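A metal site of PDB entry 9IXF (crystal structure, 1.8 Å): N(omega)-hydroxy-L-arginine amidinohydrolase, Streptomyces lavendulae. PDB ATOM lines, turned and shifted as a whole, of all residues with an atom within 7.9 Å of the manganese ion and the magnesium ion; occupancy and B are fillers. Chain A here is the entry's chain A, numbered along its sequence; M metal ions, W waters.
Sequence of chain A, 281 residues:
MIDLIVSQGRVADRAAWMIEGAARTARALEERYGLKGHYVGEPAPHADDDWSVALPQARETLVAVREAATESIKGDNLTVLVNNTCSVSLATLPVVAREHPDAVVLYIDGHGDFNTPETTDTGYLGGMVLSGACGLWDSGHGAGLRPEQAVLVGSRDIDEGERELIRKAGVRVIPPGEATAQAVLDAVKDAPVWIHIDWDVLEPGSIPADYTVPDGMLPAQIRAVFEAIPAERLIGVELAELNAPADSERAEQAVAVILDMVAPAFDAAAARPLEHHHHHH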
ATOM      1  N   THR A  85       5.700  -6.869  16.584  1.00  0.00           N
ATOM      2  CA  THR A  85       5.468  -6.096  17.804  1.00  0.00           C
ATOM      3  C   THR A  85       6.485  -4.972  17.967  1.00  0.00           C
ATOM      4  O   THR A  85       7.576  -4.986  17.388  1.00  0.00           O
ATOM      5  CB  THR A  85       5.548  -6.949  19.082  1.00  0.00           C
ATOM      6  OG1 THR A  85       6.839  -7.545  19.177  1.00  0.00           O
ATOM      7  CG2 THR A  85       4.495  -8.057  19.079  1.00  0.00           C
ATOM      8  N   CYS A  86       6.108  -4.002  18.802  1.00  0.00           N
ATOM      9  CA  CYS A  86       7.038  -2.933  19.150  1.00  0.00           C
ATOM     10  C   CYS A  86       8.309  -3.476  19.804  1.00  0.00           C
ATOM     11  O   CYS A  86       9.371  -2.858  19.719  1.00  0.00           O
ATOM     12  CB  CYS A  86       6.362  -1.939  20.111  1.00  0.00           C
ATOM     13  SG  CYS A  86       5.173  -0.803  19.256  1.00  0.00           S
ATOM     14  N   SER A  87       8.204  -4.647  20.451  1.00  0.00           N
ATOM     15  CA  SER A  87       9.327  -5.205  21.185  1.00  0.00           C
ATOM     16  C   SER A  87      10.514  -5.513  20.292  1.00  0.00           C
ATOM     17  O   SER A  87      11.638  -5.609  20.784  1.00  0.00           O
ATOM     18  CB  SER A  87       8.908  -6.474  21.906  1.00  0.00           C
ATOM     19  OG  SER A  87       7.932  -6.153  22.884  1.00  0.00           O
ATOM     20  N   TYR A 107       8.676   8.201  18.281  1.00  0.00           N
ATOM     21  CA  TYR A 107       8.067   6.956  18.714  1.00  0.00           C
ATOM     22  C   TYR A 107       6.567   7.228  18.727  1.00  0.00           C
ATOM     23  O   TYR A 107       6.025   7.810  19.680  1.00  0.00           O
ATOM     24  CB  TYR A 107       8.647   6.543  20.072  1.00  0.00           C
ATOM     25  CG  TYR A 107       8.385   5.086  20.451  1.00  0.00           C
ATOM     26  CD1 TYR A 107       7.149   4.699  20.935  1.00  0.00           C
ATOM     27  CD2 TYR A 107       9.371   4.139  20.334  1.00  0.00           C
ATOM     28  CE1 TYR A 107       6.892   3.368  21.287  1.00  0.00           C
ATOM     29  CE2 TYR A 107       9.128   2.783  20.679  1.00  0.00           C
ATOM     30  CZ  TYR A 107       7.889   2.419  21.158  1.00  0.00           C
ATOM     31  OH  TYR A 107       7.622   1.091  21.509  1.00  0.00           O
ATOM     32  N   ILE A 108       5.888   6.842  17.627  1.00  0.00           N
ATOM     33  CA  ILE A 108       4.501   7.199  17.389  1.00  0.00           C
ATOM     34  C   ILE A 108       3.640   6.040  17.865  1.00  0.00           C
ATOM     35  O   ILE A 108       3.715   4.950  17.305  1.00  0.00           O
ATOM     36  CB  ILE A 108       4.258   7.483  15.896  1.00  0.00           C
ATOM     37  CG1 ILE A 108       5.339   8.424  15.369  1.00  0.00           C
ATOM     38  CG2 ILE A 108       2.841   8.013  15.672  1.00  0.00           C
ATOM     39  CD1 ILE A 108       5.113   8.894  13.955  1.00  0.00           C
ATOM     40  N   ASP A 109       2.844   6.281  18.905  1.00  0.00           N
ATOM     41  CA  ASP A 109       2.244   5.165  19.648  1.00  0.00           C
ATOM     42  C   ASP A 109       1.122   5.740  20.480  1.00  0.00           C
ATOM     43  O   ASP A 109       1.237   6.856  20.975  1.00  0.00           O
ATOM     44  CB  ASP A 109       3.312   4.509  20.547  1.00  0.00           C
ATOM     45  CG  ASP A 109       2.942   3.102  20.986  1.00  0.00           C
ATOM     46  OD1 ASP A 109       1.795   2.880  21.428  1.00  0.00           O
ATOM     47  OD2 ASP A 109       3.821   2.242  20.911  1.00  0.00           O
ATOM     48  N   GLY A 110       0.007   5.002  20.579  1.00  0.00           N
ATOM     49  CA  GLY A 110      -1.032   5.422  21.520  1.00  0.00           C
ATOM     50  C   GLY A 110      -0.580   5.362  22.962  1.00  0.00           C
ATOM     51  O   GLY A 110      -1.162   6.035  23.829  1.00  0.00           O
ATOM     52  N   HIS A 111       0.436   4.551  23.251  1.00  0.00           N
ATOM     53  CA  HIS A 111       1.017   4.326  24.556  1.00  0.00           C
ATOM     54  C   HIS A 111       2.387   4.980  24.672  1.00  0.00           C
ATOM     55  O   HIS A 111       2.972   5.443  23.692  1.00  0.00           O
ATOM     56  CB  HIS A 111       1.145   2.824  24.791  1.00  0.00           C
ATOM     57  CG  HIS A 111      -0.148   2.082  24.623  1.00  0.00           C
ATOM     58  ND1 HIS A 111      -0.547   1.528  23.427  1.00  0.00           N
ATOM     59  CD2 HIS A 111      -1.111   1.771  25.527  1.00  0.00           C
ATOM     60  CE1 HIS A 111      -1.702   0.910  23.600  1.00  0.00           C
ATOM     61  NE2 HIS A 111      -2.080   1.056  24.860  1.00  0.00           N
ATOM     62  N   GLY A 112       2.908   5.012  25.900  1.00  0.00           N
ATOM     63  CA  GLY A 112       4.255   5.495  26.108  1.00  0.00           C
ATOM     64  C   GLY A 112       5.324   4.419  25.973  1.00  0.00           C
ATOM     65  O   GLY A 112       6.496   4.748  25.726  1.00  0.00           O
ATOM     66  N   ASP A 113       4.945   3.154  26.177  1.00  0.00           N
ATOM     67  CA  ASP A 113       5.899   2.020  26.101  1.00  0.00           C
ATOM     68  C   ASP A 113       7.152   2.298  26.934  1.00  0.00           C
ATOM     69  O   ASP A 113       8.281   1.961  26.568  1.00  0.00           O
ATOM     70  CB  ASP A 113       6.263   1.655  24.646  1.00  0.00           C
ATOM     71  CG  ASP A 113       5.089   1.029  23.887  1.00  0.00           C
ATOM     72  OD1 ASP A 113       3.968   0.964  24.457  1.00  0.00           O
ATOM     73  OD2 ASP A 113       5.285   0.613  22.700  1.00  0.00           O
ATOM     74  N   TYR A 124       3.998  -6.900  30.308  1.00  0.00           N
ATOM     75  CA  TYR A 124       4.085  -7.052  28.859  1.00  0.00           C
ATOM     76  C   TYR A 124       5.364  -6.381  28.356  1.00  0.00           C
ATOM     77  O   TYR A 124       5.563  -5.185  28.566  1.00  0.00           O
ATOM     78  CB  TYR A 124       2.854  -6.443  28.186  1.00  0.00           C
ATOM     79  CG  TYR A 124       2.872  -6.515  26.690  1.00  0.00           C
ATOM     80  CD1 TYR A 124       3.331  -7.660  26.019  1.00  0.00           C
ATOM     81  CD2 TYR A 124       2.447  -5.437  25.924  1.00  0.00           C
ATOM     82  CE1 TYR A 124       3.336  -7.726  24.651  1.00  0.00           C
ATOM     83  CE2 TYR A 124       2.470  -5.485  24.538  1.00  0.00           C
ATOM     84  CZ  TYR A 124       2.908  -6.613  23.908  1.00  0.00           C
ATOM     85  OH  TYR A 124       2.919  -6.615  22.538  1.00  0.00           O
ATOM     86  N   GLY A 126       6.111  -5.470  25.433  1.00  0.00           N
ATOM     87  CA  GLY A 126       5.783  -4.414  24.493  1.00  0.00           C
ATOM     88  C   GLY A 126       5.503  -3.076  25.128  1.00  0.00           C
ATOM     89  O   GLY A 126       5.523  -2.055  24.432  1.00  0.00           O
ATOM     90  N   GLY A 127       5.186  -3.043  26.425  1.00  0.00           N
ATOM     91  CA  GLY A 127       5.062  -1.787  27.140  1.00  0.00           C
ATOM     92  C   GLY A 127       6.339  -1.300  27.782  1.00  0.00           C
ATOM     93  O   GLY A 127       6.289  -0.338  28.552  1.00  0.00           O
ATOM     94  N   MET A 128       7.492  -1.925  27.472  1.00  0.00           N
ATOM     95  CA  MET A 128       8.794  -1.632  28.091  1.00  0.00           C
ATOM     96  C   MET A 128       9.866  -1.277  27.062  1.00  0.00           C
ATOM     97  O   MET A 128      11.065  -1.280  27.376  1.00  0.00           O
ATOM     98  CB  MET A 128       9.239  -2.840  28.937  1.00  0.00           C
ATOM     99  CG  MET A 128       8.172  -3.317  29.923  1.00  0.00           C
ATOM    100  SD  MET A 128       8.473  -4.986  30.620  1.00  0.00           S
ATOM    101  CE  MET A 128      10.030  -4.702  31.444  1.00  0.00           C
ATOM    102  N   VAL A 129       9.454  -0.925  25.829  1.00  0.00           N
ATOM    103  CA  VAL A 129      10.374  -0.850  24.683  1.00  0.00           C
ATOM    104  C   VAL A 129      11.208   0.428  24.711  1.00  0.00           C
ATOM    105  O   VAL A 129      12.431   0.366  24.589  1.00  0.00           O
ATOM    106  CB  VAL A 129       9.586  -0.952  23.358  1.00  0.00           C
ATOM    107  CG1 VAL A 129      10.524  -0.745  22.165  1.00  0.00           C
ATOM    108  CG2 VAL A 129       8.908  -2.298  23.268  1.00  0.00           C
ATOM    109  N   LEU A 130      10.553   1.597  24.793  1.00  0.00           N
ATOM    110  CA  LEU A 130      11.305   2.844  24.736  1.00  0.00           C
ATOM    111  C   LEU A 130      12.165   3.025  25.976  1.00  0.00           C
ATOM    112  O   LEU A 130      13.292   3.532  25.885  1.00  0.00           O
ATOM    113  CB  LEU A 130      10.354   4.032  24.544  1.00  0.00           C
ATOM    114  CG  LEU A 130      10.975   5.410  24.300  1.00  0.00           C
ATOM    115  CD1 LEU A 130      11.903   5.359  23.076  1.00  0.00           C
ATOM    116  CD2 LEU A 130       9.851   6.444  24.097  1.00  0.00           C
ATOM    117  N   SER A 155       0.778   9.793  21.940  1.00  0.00           N
ATOM    118  CA  SER A 155       0.488   9.045  23.154  1.00  0.00           C
ATOM    119  C   SER A 155      -0.527   9.804  24.005  1.00  0.00           C
ATOM    120  O   SER A 155      -0.538  11.032  24.040  1.00  0.00           O
ATOM    121  CB  SER A 155       1.764   8.830  23.951  1.00  0.00           C
ATOM    122  OG  SER A 155       2.800   8.426  23.075  1.00  0.00           O
ATOM    123  N   HIS A 196       9.326   5.272  14.405  1.00  0.00           N
ATOM    124  CA  HIS A 196       8.781   4.007  14.874  1.00  0.00           C
ATOM    125  C   HIS A 196       7.278   4.208  15.025  1.00  0.00           C
ATOM    126  O   HIS A 196       6.882   5.129  15.732  1.00  0.00           O
ATOM    127  CB  HIS A 196       9.444   3.628  16.209  1.00  0.00           C
ATOM    128  CG  HIS A 196       8.763   2.511  16.933  1.00  0.00           C
ATOM    129  ND1 HIS A 196       9.341   1.265  17.079  1.00  0.00           N
ATOM    130  CD2 HIS A 196       7.571   2.442  17.565  1.00  0.00           C
ATOM    131  CE1 HIS A 196       8.519   0.473  17.756  1.00  0.00           C
ATOM    132  NE2 HIS A 196       7.439   1.177  18.060  1.00  0.00           N
ATOM    133  N   ILE A 197       6.447   3.386  14.369  1.00  0.00           N
ATOM    134  CA  ILE A 197       4.986   3.529  14.472  1.00  0.00           C
ATOM    135  C   ILE A 197       4.358   2.250  15.000  1.00  0.00           C
ATOM    136  O   ILE A 197       4.571   1.170  14.444  1.00  0.00           O
ATOM    137  CB  ILE A 197       4.338   3.884  13.130  1.00  0.00           C
ATOM    138  CG1 ILE A 197       5.094   5.023  12.445  1.00  0.00           C
ATOM    139  CG2 ILE A 197       2.864   4.243  13.381  1.00  0.00           C
ATOM    140  CD1 ILE A 197       4.538   5.364  11.079  1.00  0.00           C
ATOM    141  N   ASP A 198       3.541   2.408  16.046  1.00  0.00           N
ATOM    142  CA  ASP A 198       2.619   1.387  16.545  1.00  0.00           C
ATOM    143  C   ASP A 198       1.217   1.790  16.087  1.00  0.00           C
ATOM    144  O   ASP A 198       0.744   2.891  16.417  1.00  0.00           O
ATOM    145  CB  ASP A 198       2.733   1.343  18.073  1.00  0.00           C
ATOM    146  CG  ASP A 198       1.724   0.428  18.753  1.00  0.00           C
ATOM    147  OD1 ASP A 198       0.769  -0.058  18.117  1.00  0.00           O
ATOM    148  OD2 ASP A 198       1.910   0.205  19.978  1.00  0.00           O
ATOM    149  N   TRP A 199       0.553   0.923  15.322  1.00  0.00           N
ATOM    150  CA  TRP A 199      -0.708   1.364  14.712  1.00  0.00           C
ATOM    151  C   TRP A 199      -1.814   1.640  15.728  1.00  0.00           C
ATOM    152  O   TRP A 199      -2.816   2.259  15.350  1.00  0.00           O
ATOM    153  CB  TRP A 199      -1.176   0.354  13.642  1.00  0.00           C
ATOM    154  CG  TRP A 199      -0.198   0.248  12.485  1.00  0.00           C
ATOM    155  CD1 TRP A 199       0.475  -0.873  12.087  1.00  0.00           C
ATOM    156  CD2 TRP A 199       0.259   1.310  11.606  1.00  0.00           C
ATOM    157  NE1 TRP A 199       1.292  -0.591  11.026  1.00  0.00           N
ATOM    158  CE2 TRP A 199       1.192   0.743  10.720  1.00  0.00           C
ATOM    159  CE3 TRP A 199      -0.041   2.682  11.497  1.00  0.00           C
ATOM    160  CZ2 TRP A 199       1.830   1.487   9.723  1.00  0.00           C
ATOM    161  CZ3 TRP A 199       0.605   3.422  10.515  1.00  0.00           C
ATOM    162  CH2 TRP A 199       1.528   2.820   9.633  1.00  0.00           C
ATOM    163  N   ASP A 200      -1.655   1.251  17.003  1.00  0.00           N
ATOM    164  CA  ASP A 200      -2.700   1.650  17.949  1.00  0.00           C
ATOM    165  C   ASP A 200      -2.700   3.152  18.224  1.00  0.00           C
ATOM    166  O   ASP A 200      -3.583   3.629  18.932  1.00  0.00           O
ATOM    167  CB  ASP A 200      -2.621   0.852  19.273  1.00  0.00           C
ATOM    168  CG  ASP A 200      -1.324   1.048  20.078  1.00  0.00           C
ATOM    169  OD1 ASP A 200      -0.728   2.141  20.048  1.00  0.00           O
ATOM    170  OD2 ASP A 200      -0.934   0.100  20.804  1.00  0.00           O
ATOM    171  N   VAL A 201      -1.781   3.919  17.637  1.00  0.00           N
ATOM    172  CA  VAL A 201      -1.883   5.378  17.710  1.00  0.00           C
ATOM    173  C   VAL A 201      -3.109   5.890  16.960  1.00  0.00           C
ATOM    174  O   VAL A 201      -3.599   6.990  17.267  1.00  0.00           O
ATOM    175  CB  VAL A 201      -0.595   6.021  17.164  1.00  0.00           C
ATOM    176  CG1 VAL A 201      -0.525   5.932  15.638  1.00  0.00           C
ATOM    177  CG2 VAL A 201      -0.473   7.487  17.653  1.00  0.00           C
ATOM    178  N   ALA A 240       4.836  -1.317  13.097  1.00  0.00           N
ATOM    179  CA  ALA A 240       4.582  -2.407  14.044  1.00  0.00           C
ATOM    180  C   ALA A 240       3.122  -2.490  14.454  1.00  0.00           C
ATOM    181  O   ALA A 240       2.421  -1.481  14.491  1.00  0.00           O
ATOM    182  CB  ALA A 240       5.441  -2.214  15.313  1.00  0.00           C
ATOM    183  N   GLU A 241       2.678  -3.708  14.782  1.00  0.00           N
ATOM    184  CA  GLU A 241       1.460  -3.986  15.540  1.00  0.00           C
ATOM    185  C   GLU A 241       0.182  -3.796  14.698  1.00  0.00           C
ATOM    186  O   GLU A 241      -0.782  -3.180  15.153  1.00  0.00           O
ATOM    187  CB  GLU A 241       1.440  -3.126  16.821  1.00  0.00           C
ATOM    188  CG  GLU A 241       2.738  -3.357  17.656  1.00  0.00           C
ATOM    189  CD  GLU A 241       2.531  -3.655  19.154  1.00  0.00           C
ATOM    190  OE1 GLU A 241       1.389  -3.548  19.660  1.00  0.00           O
ATOM    191  OE2 GLU A 241       3.549  -3.957  19.840  1.00  0.00           O
HETATM  192 MN    MN M   1       3.819   0.089  21.179  1.00  0.00          MN
HETATM  193 MG    MG M   2       0.688   1.166  21.544  1.00  0.00          MG
HETATM  194  O   HOH W   1       2.090   0.103  22.696  1.00  0.00           O
HETATM  195  O   HOH W   2       3.684  -1.912  21.869  1.00  0.00           O
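Of the 25 residues printed, 4 come within 4 Å of the magnesium ion.
OH of Tyr 107 touches the manganese ion, 3.9 Å away.
Within 4 Å of the manganese ion: Cys 86, Tyr 107, Asp 109, Asp 113 and Asp 198.
The nearest printed residue that does not touch the manganese ion is Gly 126 (4.3 Å).
Water W2 binds the manganese ion (2.1 Å).
OD2 of Asp 109 is bound to the manganese ion (2.2 Å).
OD2 of Asp 113 is bound to the manganese ion (2.2 Å).
The side-chain carboxylate (OD2) of Asp 198 binds the manganese ion, at 2.3 Å.
The manganese ion is bound by water W1, at 2.3 Å.
SG of Cys 86 is bound to the manganese ion (2.5 Å).
OD1 of Asp 109 is bound to the magnesium ion (2.0 Å).
OD2 of Asp 200 is bound to the magnesium ion (2.1 Å).
Water W1 binds the magnesium ion (2.1 Å).
The magnesium ion is bound by OD2 of Asp 198, at 2.2 Å.
OD1 of Asp 200 is bound to the magnesium ion, at 2.3 Å.
A ring nitrogen (ND1) of His 111 binds the magnesium ion, 2.3 Å away.
Water W2 lies within hydrogen-bond range of OE2 of Glu 241 and O of Gly 126.
O of Asp 109 sits at hydrogen-bond distance from OG of Ser 155 (3.1 Å).
The backbone NH of Gly 110 lies close to the side-chain carboxylate of Asp 200, at 3.0 Å.
The backbone carbonyl oxygen (O) of Asp 113 lies within hydrogen-bond range of the backbone NH (N) of Val 129 (3.2 Å).
N of Asp 198 is in hydrogen-bond range of O of Ile 108.
The backbone carbonyl oxygen (O) of His 111 is in hydrogen-bond range of the side-chain hydroxyl (OG) of Ser 155.
N of Cys 86 lies within hydrogen-bond range of OE2 of Glu 241 (2.8 Å).
The side-chain sulfur (SG) of Cys 86 lies close to a ring nitrogen (NE2) of His 196.
OH of Tyr 107 sits close to NE2 of His 196, 3.5 Å away.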
